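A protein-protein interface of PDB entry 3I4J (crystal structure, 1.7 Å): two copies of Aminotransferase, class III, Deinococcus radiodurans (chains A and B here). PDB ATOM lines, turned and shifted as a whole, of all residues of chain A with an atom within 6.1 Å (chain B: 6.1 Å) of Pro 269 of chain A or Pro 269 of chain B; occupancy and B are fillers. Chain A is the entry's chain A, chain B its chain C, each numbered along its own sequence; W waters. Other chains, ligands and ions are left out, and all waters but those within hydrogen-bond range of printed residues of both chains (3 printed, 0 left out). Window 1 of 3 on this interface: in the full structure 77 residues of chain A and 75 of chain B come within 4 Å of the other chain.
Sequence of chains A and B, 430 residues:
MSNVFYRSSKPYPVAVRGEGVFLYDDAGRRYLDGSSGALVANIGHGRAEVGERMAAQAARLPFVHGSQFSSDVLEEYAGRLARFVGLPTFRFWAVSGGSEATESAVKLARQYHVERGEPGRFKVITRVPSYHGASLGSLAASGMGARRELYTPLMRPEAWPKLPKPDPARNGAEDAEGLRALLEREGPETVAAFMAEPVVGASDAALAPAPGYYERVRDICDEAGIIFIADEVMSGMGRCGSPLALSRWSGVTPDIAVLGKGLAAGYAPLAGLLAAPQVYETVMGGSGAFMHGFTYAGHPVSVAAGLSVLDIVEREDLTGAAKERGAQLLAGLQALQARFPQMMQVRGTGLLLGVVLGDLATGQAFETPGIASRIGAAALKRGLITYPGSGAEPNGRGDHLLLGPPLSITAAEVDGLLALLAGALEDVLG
Water W3 lies within hydrogen-bond range of the backbone carbonyl oxygen of Leu 270 of chain B (2.7 Å), the side-chain hydroxyl of Tyr 296 of chain A (2.9 Å), the backbone NH of Ala 264 of chain B (2.9 Å) and the backbone carbonyl oxygen of Ala 268 of chain B (3.5 Å).
Water W1 lies within hydrogen-bond range of the backbone carbonyl oxygen (O) of Leu 270 of chain A, the backbone NH (N) of Ala 264 of chain A and the side-chain hydroxyl (OH) of Tyr 296 of chain B.
Water W2 lies within hydrogen-bond range of O of Ser 96 of chain A and OG of Ser 96 of chain B.
The backbone carbonyl oxygen of Ala 268 of chain B sits at hydrogen-bond distance from the side-chain hydroxyl of Tyr 296 of chain A, at 3.2 Å.
The backbone carbonyl oxygen of Tyr 267 of chain B lies within hydrogen-bond range of a ring nitrogen (NE2) of His 299 of chain A (3.2 Å).
NE2 of His 299 of chain B sits at hydrogen-bond distance from O of Tyr 267 of chain A, at 3.2 Å.
O of Ala 268 of chain A lies within hydrogen-bond range of OH of Tyr 296 of chain B (3.0 Å).
Tyr 267 of chain A touches His 299 of chain B, and with the chains exchanged His 299 of chain A touches Tyr 267 of chain B.
Pro 269 of chain B touches its own counterpart, Pro 269 of chain A.
Pro 269 of chain A touches His 299 of chain B, and with the chains exchanged His 299 of chain A touches Pro 269 of chain B.
Pro 269 of chain A touches Ser 302 of chain B, and with the chains exchanged Ser 302 of chain A touches Pro 269 of chain B.
Of the 13 pairs that touch across the chains among the printed residues, 13 have their exchanged pair printed and touching as well.
His 299 of chain B touches Ala 268 of chain A.
CD of Pro 269 of chain A touches CD of Pro 269 of chain B, at 3.7 Å.
Tyr 296 of chain B touches Pro 269 of chain A (CD2 to CA, 3.7 Å).
Pro 269 of chain A touches His 299 of chain B.
OG of Ser 302 of chain B touches CD of Pro 269 of chain A (3.6 Å).
Tyr 296 of chain A touches Pro 269 of chain B (CG to CA, 3.9 Å).
Ala 268 of chain B touches His 299 of chain A (N to NE2, 3.6 Å).
Pro 269 of chain B touches His 299 of chain A (CD to CD2, 3.8 Å).
OG of Ser 302 of chain A touches CD of Pro 269 of chain B, 3.6 Å away.
Of chain B, only Pro 269 (3.7 Å), Tyr 296 (3.7 Å), His 299 (3.8 Å) and Ser 302 (3.6 Å) come within 4 Å of Pro 269 of chain A.
Of chain A, only Pro 269, Tyr 296, His 299 and Ser 302 come within 4 Å of Pro 269 of chain B.
Printed residues of chain B within 4 Å of His 299 of chain A: Tyr 267, Ala 268 and Pro 269.
Printed residues of chain A within 4 Å of Ser 302 of chain B: Pro 269 (3.6 Å).
Of the printed residues of chain B, Tyr 267 of chain A touches His 299 (3.2 Å).
Of the printed residues of chain B, Ser 302 of chain A touches Pro 269 (3.6 Å).
Of the printed residues of chain A, His 299 of chain B touches Tyr 267 (3.2 Å), Ala 268 (3.6 Å) and Pro 269 (3.8 Å).
Gly 97 of chain B touches none of the printed residues of chain A.
Ala 271 of chain A touches none of the printed residues of chain B.
The nearest residue of chain A that does not touch Pro 269 of chain B is Ser 96 of chain A (4.2 Å).
Printed residues of chain B that touch a printed residue of chain A: Tyr 267, Ala 268, Pro 269, Tyr 296, His 299 and Ser 302.
Hydrophobic or aromatic side chains of chain B within 4 Å of the printed part of chain A: Pro 269, Tyr 296 and His 299.
Of the 12 printed residues of chain A, 6 touch a printed residue of chain B.
Hydrophobic or aromatic side chains of chain A that line the printed part of chain B: Pro 269, Tyr 296 and His 299.
Among the printed residues, 13 pairs touch across the chains.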
ATOM      1  N   VAL A  95      12.530  30.850 -13.508  1.00  0.00           N
ATOM      2  CA  VAL A  95      12.817  30.113 -14.736  1.00  0.00           C
ATOM      3  C   VAL A  95      12.125  28.756 -14.626  1.00  0.00           C
ATOM      4  O   VAL A  95      11.381  28.522 -13.673  1.00  0.00           O
ATOM      5  CB  VAL A  95      14.337  29.943 -14.975  1.00  0.00           C
ATOM      6  CG1 VAL A  95      14.976  31.313 -15.147  1.00  0.00           C
ATOM      7  CG2 VAL A  95      14.986  29.196 -13.823  1.00  0.00           C
ATOM      8  N   SER A  96      12.360  27.850 -15.571  1.00  0.00           N
ATOM      9  CA  SER A  96      11.654  26.571 -15.525  1.00  0.00           C
ATOM     10  C   SER A  96      12.412  25.329 -15.065  1.00  0.00           C
ATOM     11  O   SER A  96      11.803  24.272 -14.871  1.00  0.00           O
ATOM     12  CB  SER A  96      11.025  26.290 -16.894  1.00  0.00           C
ATOM     13  OG  SER A  96      10.168  27.355 -17.283  1.00  0.00           O
ATOM     14  N   GLY A  97      13.725  25.446 -14.893  1.00  0.00           N
ATOM     15  CA  GLY A  97      14.514  24.302 -14.462  1.00  0.00           C
ATOM     16  C   GLY A  97      15.789  24.701 -13.745  1.00  0.00           C
ATOM     17  O   GLY A  97      16.251  25.832 -13.885  1.00  0.00           O
ATOM     18  N   ALA A 264       8.452  23.831  -6.664  1.00  0.00           N
ATOM     19  CA  ALA A 264       7.083  23.460  -6.997  1.00  0.00           C
ATOM     20  C   ALA A 264       6.885  21.985  -6.629  1.00  0.00           C
ATOM     21  O   ALA A 264       5.847  21.393  -6.906  1.00  0.00           O
ATOM     22  CB  ALA A 264       6.804  23.694  -8.482  1.00  0.00           C
ATOM     23  N   TYR A 267       5.182  19.518  -8.979  1.00  0.00           N
ATOM     24  CA  TYR A 267       3.877  19.858  -9.535  1.00  0.00           C
ATOM     25  C   TYR A 267       3.953  20.711 -10.795  1.00  0.00           C
ATOM     26  O   TYR A 267       3.002  20.754 -11.566  1.00  0.00           O
ATOM     27  CB  TYR A 267       3.014  20.526  -8.460  1.00  0.00           C
ATOM     28  CG  TYR A 267       2.531  19.500  -7.467  1.00  0.00           C
ATOM     29  CD1 TYR A 267       1.392  18.732  -7.727  1.00  0.00           C
ATOM     30  CD2 TYR A 267       3.290  19.189  -6.342  1.00  0.00           C
ATOM     31  CE1 TYR A 267       1.030  17.671  -6.891  1.00  0.00           C
ATOM     32  CE2 TYR A 267       2.939  18.129  -5.504  1.00  0.00           C
ATOM     33  CZ  TYR A 267       1.814  17.374  -5.789  1.00  0.00           C
ATOM     34  OH  TYR A 267       1.501  16.291  -4.990  1.00  0.00           O
ATOM     35  N   ALA A 268       5.095  21.371 -11.000  1.00  0.00           N
ATOM     36  CA  ALA A 268       5.319  22.204 -12.182  1.00  0.00           C
ATOM     37  C   ALA A 268       6.816  22.447 -12.360  1.00  0.00           C
ATOM     38  O   ALA A 268       7.565  22.433 -11.387  1.00  0.00           O
ATOM     39  CB  ALA A 268       4.598  23.545 -12.036  1.00  0.00           C
ATOM     40  N   PRO A 269       7.277  22.640 -13.614  1.00  0.00           N
ATOM     41  CA  PRO A 269       8.706  22.892 -13.832  1.00  0.00           C
ATOM     42  C   PRO A 269       8.957  24.328 -13.375  1.00  0.00           C
ATOM     43  O   PRO A 269       8.627  25.284 -14.082  1.00  0.00           O
ATOM     44  CB  PRO A 269       8.870  22.732 -15.351  1.00  0.00           C
ATOM     45  CG  PRO A 269       7.681  21.875 -15.754  1.00  0.00           C
ATOM     46  CD  PRO A 269       6.580  22.445 -14.897  1.00  0.00           C
ATOM     47  N   LEU A 270       9.521  24.474 -12.185  1.00  0.00           N
ATOM     48  CA  LEU A 270       9.775  25.798 -11.635  1.00  0.00           C
ATOM     49  C   LEU A 270      11.106  25.834 -10.905  1.00  0.00           C
ATOM     50  O   LEU A 270      11.436  24.919 -10.152  1.00  0.00           O
ATOM     51  CB  LEU A 270       8.646  26.184 -10.667  1.00  0.00           C
ATOM     52  CG  LEU A 270       8.762  27.558  -9.997  1.00  0.00           C
ATOM     53  CD1 LEU A 270       8.581  28.642 -11.039  1.00  0.00           C
ATOM     54  CD2 LEU A 270       7.697  27.693  -8.907  1.00  0.00           C
ATOM     55  N   ALA A 271      11.861  26.899 -11.141  1.00  0.00           N
ATOM     56  CA  ALA A 271      13.152  27.103 -10.496  1.00  0.00           C
ATOM     57  C   ALA A 271      13.420  28.598 -10.510  1.00  0.00           C
ATOM     58  O   ALA A 271      12.603  29.378 -10.987  1.00  0.00           O
ATOM     59  CB  ALA A 271      14.258  26.366 -11.252  1.00  0.00           C
ATOM     60  N   TYR A 296       9.130  30.352 -20.960  1.00  0.00           N
ATOM     61  CA  TYR A 296       8.245  30.108 -19.830  1.00  0.00           C
ATOM     62  C   TYR A 296       8.717  30.665 -18.492  1.00  0.00           C
ATOM     63  O   TYR A 296       8.183  30.296 -17.447  1.00  0.00           O
ATOM     64  CB  TYR A 296       7.963  28.607 -19.707  1.00  0.00           C
ATOM     65  CG  TYR A 296       6.864  28.125 -20.636  1.00  0.00           C
ATOM     66  CD1 TYR A 296       5.525  28.177 -20.246  1.00  0.00           C
ATOM     67  CD2 TYR A 296       7.159  27.644 -21.915  1.00  0.00           C
ATOM     68  CE1 TYR A 296       4.505  27.765 -21.104  1.00  0.00           C
ATOM     69  CE2 TYR A 296       6.143  27.229 -22.782  1.00  0.00           C
ATOM     70  CZ  TYR A 296       4.820  27.291 -22.368  1.00  0.00           C
ATOM     71  OH  TYR A 296       3.812  26.864 -23.207  1.00  0.00           O
ATOM     72  N   HIS A 299       6.246  31.802 -15.772  1.00  0.00           N
ATOM     73  CA  HIS A 299       4.988  31.152 -16.145  1.00  0.00           C
ATOM     74  C   HIS A 299       3.957  31.172 -15.006  1.00  0.00           C
ATOM     75  O   HIS A 299       4.146  30.525 -13.973  1.00  0.00           O
ATOM     76  CB  HIS A 299       5.288  29.715 -16.568  1.00  0.00           C
ATOM     77  CG  HIS A 299       4.078  28.935 -16.960  1.00  0.00           C
ATOM     78  ND1 HIS A 299       3.116  29.430 -17.813  1.00  0.00           N
ATOM     79  CD2 HIS A 299       3.676  27.688 -16.621  1.00  0.00           C
ATOM     80  CE1 HIS A 299       2.169  28.523 -17.976  1.00  0.00           C
ATOM     81  NE2 HIS A 299       2.486  27.457 -17.265  1.00  0.00           N
ATOM     82  N   SER A 302       2.785  27.700 -13.387  1.00  0.00           N
ATOM     83  CA  SER A 302       3.860  27.056 -12.645  1.00  0.00           C
ATOM     84  C   SER A 302       4.149  27.830 -11.358  1.00  0.00           C
ATOM     85  O   SER A 302       4.409  27.239 -10.310  1.00  0.00           O
ATOM     86  CB  SER A 302       5.124  26.971 -13.508  1.00  0.00           C
ATOM     87  OG  SER A 302       4.903  26.146 -14.644  1.00  0.00           O
ATOM     88  N   VAL B  95      10.454  17.255 -23.300  1.00  0.00           N
ATOM     89  CA  VAL B  95      11.312  18.108 -22.484  1.00  0.00           C
ATOM     90  C   VAL B  95      10.495  19.326 -22.043  1.00  0.00           C
ATOM     91  O   VAL B  95       9.288  19.401 -22.312  1.00  0.00           O
ATOM     92  CB  VAL B  95      12.600  18.552 -23.233  1.00  0.00           C
ATOM     93  CG1 VAL B  95      13.507  17.350 -23.449  1.00  0.00           C
ATOM     94  CG2 VAL B  95      12.253  19.219 -24.557  1.00  0.00           C
ATOM     95  N   SER B  96      11.134  20.278 -21.369  1.00  0.00           N
ATOM     96  CA  SER B  96      10.419  21.445 -20.862  1.00  0.00           C
ATOM     97  C   SER B  96      10.459  22.699 -21.729  1.00  0.00           C
ATOM     98  O   SER B  96       9.576  23.549 -21.619  1.00  0.00           O
ATOM     99  CB  SER B  96      10.930  21.800 -19.462  1.00  0.00           C
ATOM    100  OG  SER B  96      10.782  20.710 -18.571  1.00  0.00           O
ATOM    101  N   GLY B  97      11.474  22.827 -22.579  1.00  0.00           N
ATOM    102  CA  GLY B  97      11.565  24.014 -23.415  1.00  0.00           C
ATOM    103  C   GLY B  97      12.110  23.780 -24.812  1.00  0.00           C
ATOM    104  O   GLY B  97      12.711  22.742 -25.096  1.00  0.00           O
ATOM    105  N   ALA B 264       1.966  23.035 -25.483  1.00  0.00           N
ATOM    106  CA  ALA B 264       1.024  23.104 -24.367  1.00  0.00           C
ATOM    107  C   ALA B 264       0.358  24.488 -24.358  1.00  0.00           C
ATOM    108  O   ALA B 264      -0.324  24.864 -23.404  1.00  0.00           O
ATOM    109  CB  ALA B 264       1.736  22.837 -23.035  1.00  0.00           C
ATOM    110  N   TYR B 267       0.020  26.740 -21.230  1.00  0.00           N
ATOM    111  CA  TYR B 267      -0.538  26.155 -20.013  1.00  0.00           C
ATOM    112  C   TYR B 267       0.486  25.414 -19.162  1.00  0.00           C
ATOM    113  O   TYR B 267       0.285  25.216 -17.965  1.00  0.00           O
ATOM    114  CB  TYR B 267      -1.720  25.244 -20.383  1.00  0.00           C
ATOM    115  CG  TYR B 267      -2.910  26.080 -20.800  1.00  0.00           C
ATOM    116  CD1 TYR B 267      -3.774  26.612 -19.841  1.00  0.00           C
ATOM    117  CD2 TYR B 267      -3.080  26.476 -22.128  1.00  0.00           C
ATOM    118  CE1 TYR B 267      -4.760  27.525 -20.181  1.00  0.00           C
ATOM    119  CE2 TYR B 267      -4.072  27.396 -22.484  1.00  0.00           C
ATOM    120  CZ  TYR B 267      -4.903  27.920 -21.499  1.00  0.00           C
ATOM    121  OH  TYR B 267      -5.847  28.877 -21.809  1.00  0.00           O
ATOM    122  N   ALA B 268       1.595  25.027 -19.779  1.00  0.00           N
ATOM    123  CA  ALA B 268       2.650  24.327 -19.068  1.00  0.00           C
ATOM    124  C   ALA B 268       3.932  24.368 -19.886  1.00  0.00           C
ATOM    125  O   ALA B 268       3.889  24.476 -21.113  1.00  0.00           O
ATOM    126  CB  ALA B 268       2.238  22.872 -18.799  1.00  0.00           C
ATOM    127  N   PRO B 269       5.094  24.304 -19.215  1.00  0.00           N
ATOM    128  CA  PRO B 269       6.365  24.330 -19.949  1.00  0.00           C
ATOM    129  C   PRO B 269       6.577  22.948 -20.561  1.00  0.00           C
ATOM    130  O   PRO B 269       7.031  22.021 -19.884  1.00  0.00           O
ATOM    131  CB  PRO B 269       7.395  24.638 -18.859  1.00  0.00           C
ATOM    132  CG  PRO B 269       6.572  25.276 -17.758  1.00  0.00           C
ATOM    133  CD  PRO B 269       5.324  24.455 -17.770  1.00  0.00           C
ATOM    134  N   LEU B 270       6.235  22.819 -21.836  1.00  0.00           N
ATOM    135  CA  LEU B 270       6.355  21.558 -22.548  1.00  0.00           C
ATOM    136  C   LEU B 270       6.898  21.782 -23.962  1.00  0.00           C
ATOM    137  O   LEU B 270       6.520  22.738 -24.647  1.00  0.00           O
ATOM    138  CB  LEU B 270       4.978  20.887 -22.629  1.00  0.00           C
ATOM    139  CG  LEU B 270       4.906  19.516 -23.306  1.00  0.00           C
ATOM    140  CD1 LEU B 270       5.592  18.487 -22.437  1.00  0.00           C
ATOM    141  CD2 LEU B 270       3.450  19.126 -23.523  1.00  0.00           C
ATOM    142  N   ALA B 271       7.789  20.889 -24.373  1.00  0.00           N
ATOM    143  CA  ALA B 271       8.417  20.918 -25.689  1.00  0.00           C
ATOM    144  C   ALA B 271       8.905  19.498 -25.945  1.00  0.00           C
ATOM    145  O   ALA B 271       8.712  18.609 -25.116  1.00  0.00           O
ATOM    146  CB  ALA B 271       9.600  21.887 -25.692  1.00  0.00           C
ATOM    147  N   TYR B 296      12.510  17.640 -15.261  1.00  0.00           N
ATOM    148  CA  TYR B 296      11.096  17.711 -15.606  1.00  0.00           C
ATOM    149  C   TYR B 296      10.724  17.171 -16.984  1.00  0.00           C
ATOM    150  O   TYR B 296       9.612  17.391 -17.452  1.00  0.00           O
ATOM    151  CB  TYR B 296      10.595  19.152 -15.440  1.00  0.00           C
ATOM    152  CG  TYR B 296      10.240  19.484 -14.002  1.00  0.00           C
ATOM    153  CD1 TYR B 296       9.015  19.095 -13.463  1.00  0.00           C
ATOM    154  CD2 TYR B 296      11.139  20.154 -13.172  1.00  0.00           C
ATOM    155  CE1 TYR B 296       8.685  19.368 -12.133  1.00  0.00           C
ATOM    156  CE2 TYR B 296      10.820  20.431 -11.832  1.00  0.00           C
ATOM    157  CZ  TYR B 296       9.591  20.036 -11.324  1.00  0.00           C
ATOM    158  OH  TYR B 296       9.245  20.326 -10.013  1.00  0.00           O
ATOM    159  N   HIS B 299       7.325  15.351 -17.520  1.00  0.00           N
ATOM    160  CA  HIS B 299       6.504  15.754 -16.375  1.00  0.00           C
ATOM    161  C   HIS B 299       5.014  15.473 -16.616  1.00  0.00           C
ATOM    162  O   HIS B 299       4.410  16.052 -17.516  1.00  0.00           O
ATOM    163  CB  HIS B 299       6.740  17.247 -16.112  1.00  0.00           C
ATOM    164  CG  HIS B 299       5.916  17.813 -14.999  1.00  0.00           C
ATOM    165  ND1 HIS B 299       5.868  17.248 -13.743  1.00  0.00           N
ATOM    166  CD2 HIS B 299       5.132  18.915 -14.947  1.00  0.00           C
ATOM    167  CE1 HIS B 299       5.088  17.979 -12.965  1.00  0.00           C
ATOM    168  NE2 HIS B 299       4.632  18.997 -13.671  1.00  0.00           N
ATOM    169  N   SER B 302       2.498  18.509 -16.885  1.00  0.00           N
ATOM    170  CA  SER B 302       2.755  19.284 -18.093  1.00  0.00           C
ATOM    171  C   SER B 302       2.308  18.508 -19.327  1.00  0.00           C
ATOM    172  O   SER B 302       1.787  19.086 -20.275  1.00  0.00           O
ATOM    173  CB  SER B 302       4.238  19.636 -18.187  1.00  0.00           C
ATOM    174  OG  SER B 302       4.594  20.528 -17.142  1.00  0.00           O
HETATM  175  O   HOH W   1      10.151  22.921  -8.910  1.00  0.00           O
HETATM  176  O   HOH W   2      12.424  22.129 -16.561  1.00  0.00           O
HETATM  177  O   HOH W   3       4.408  24.381 -24.531  1.00  0.00           O
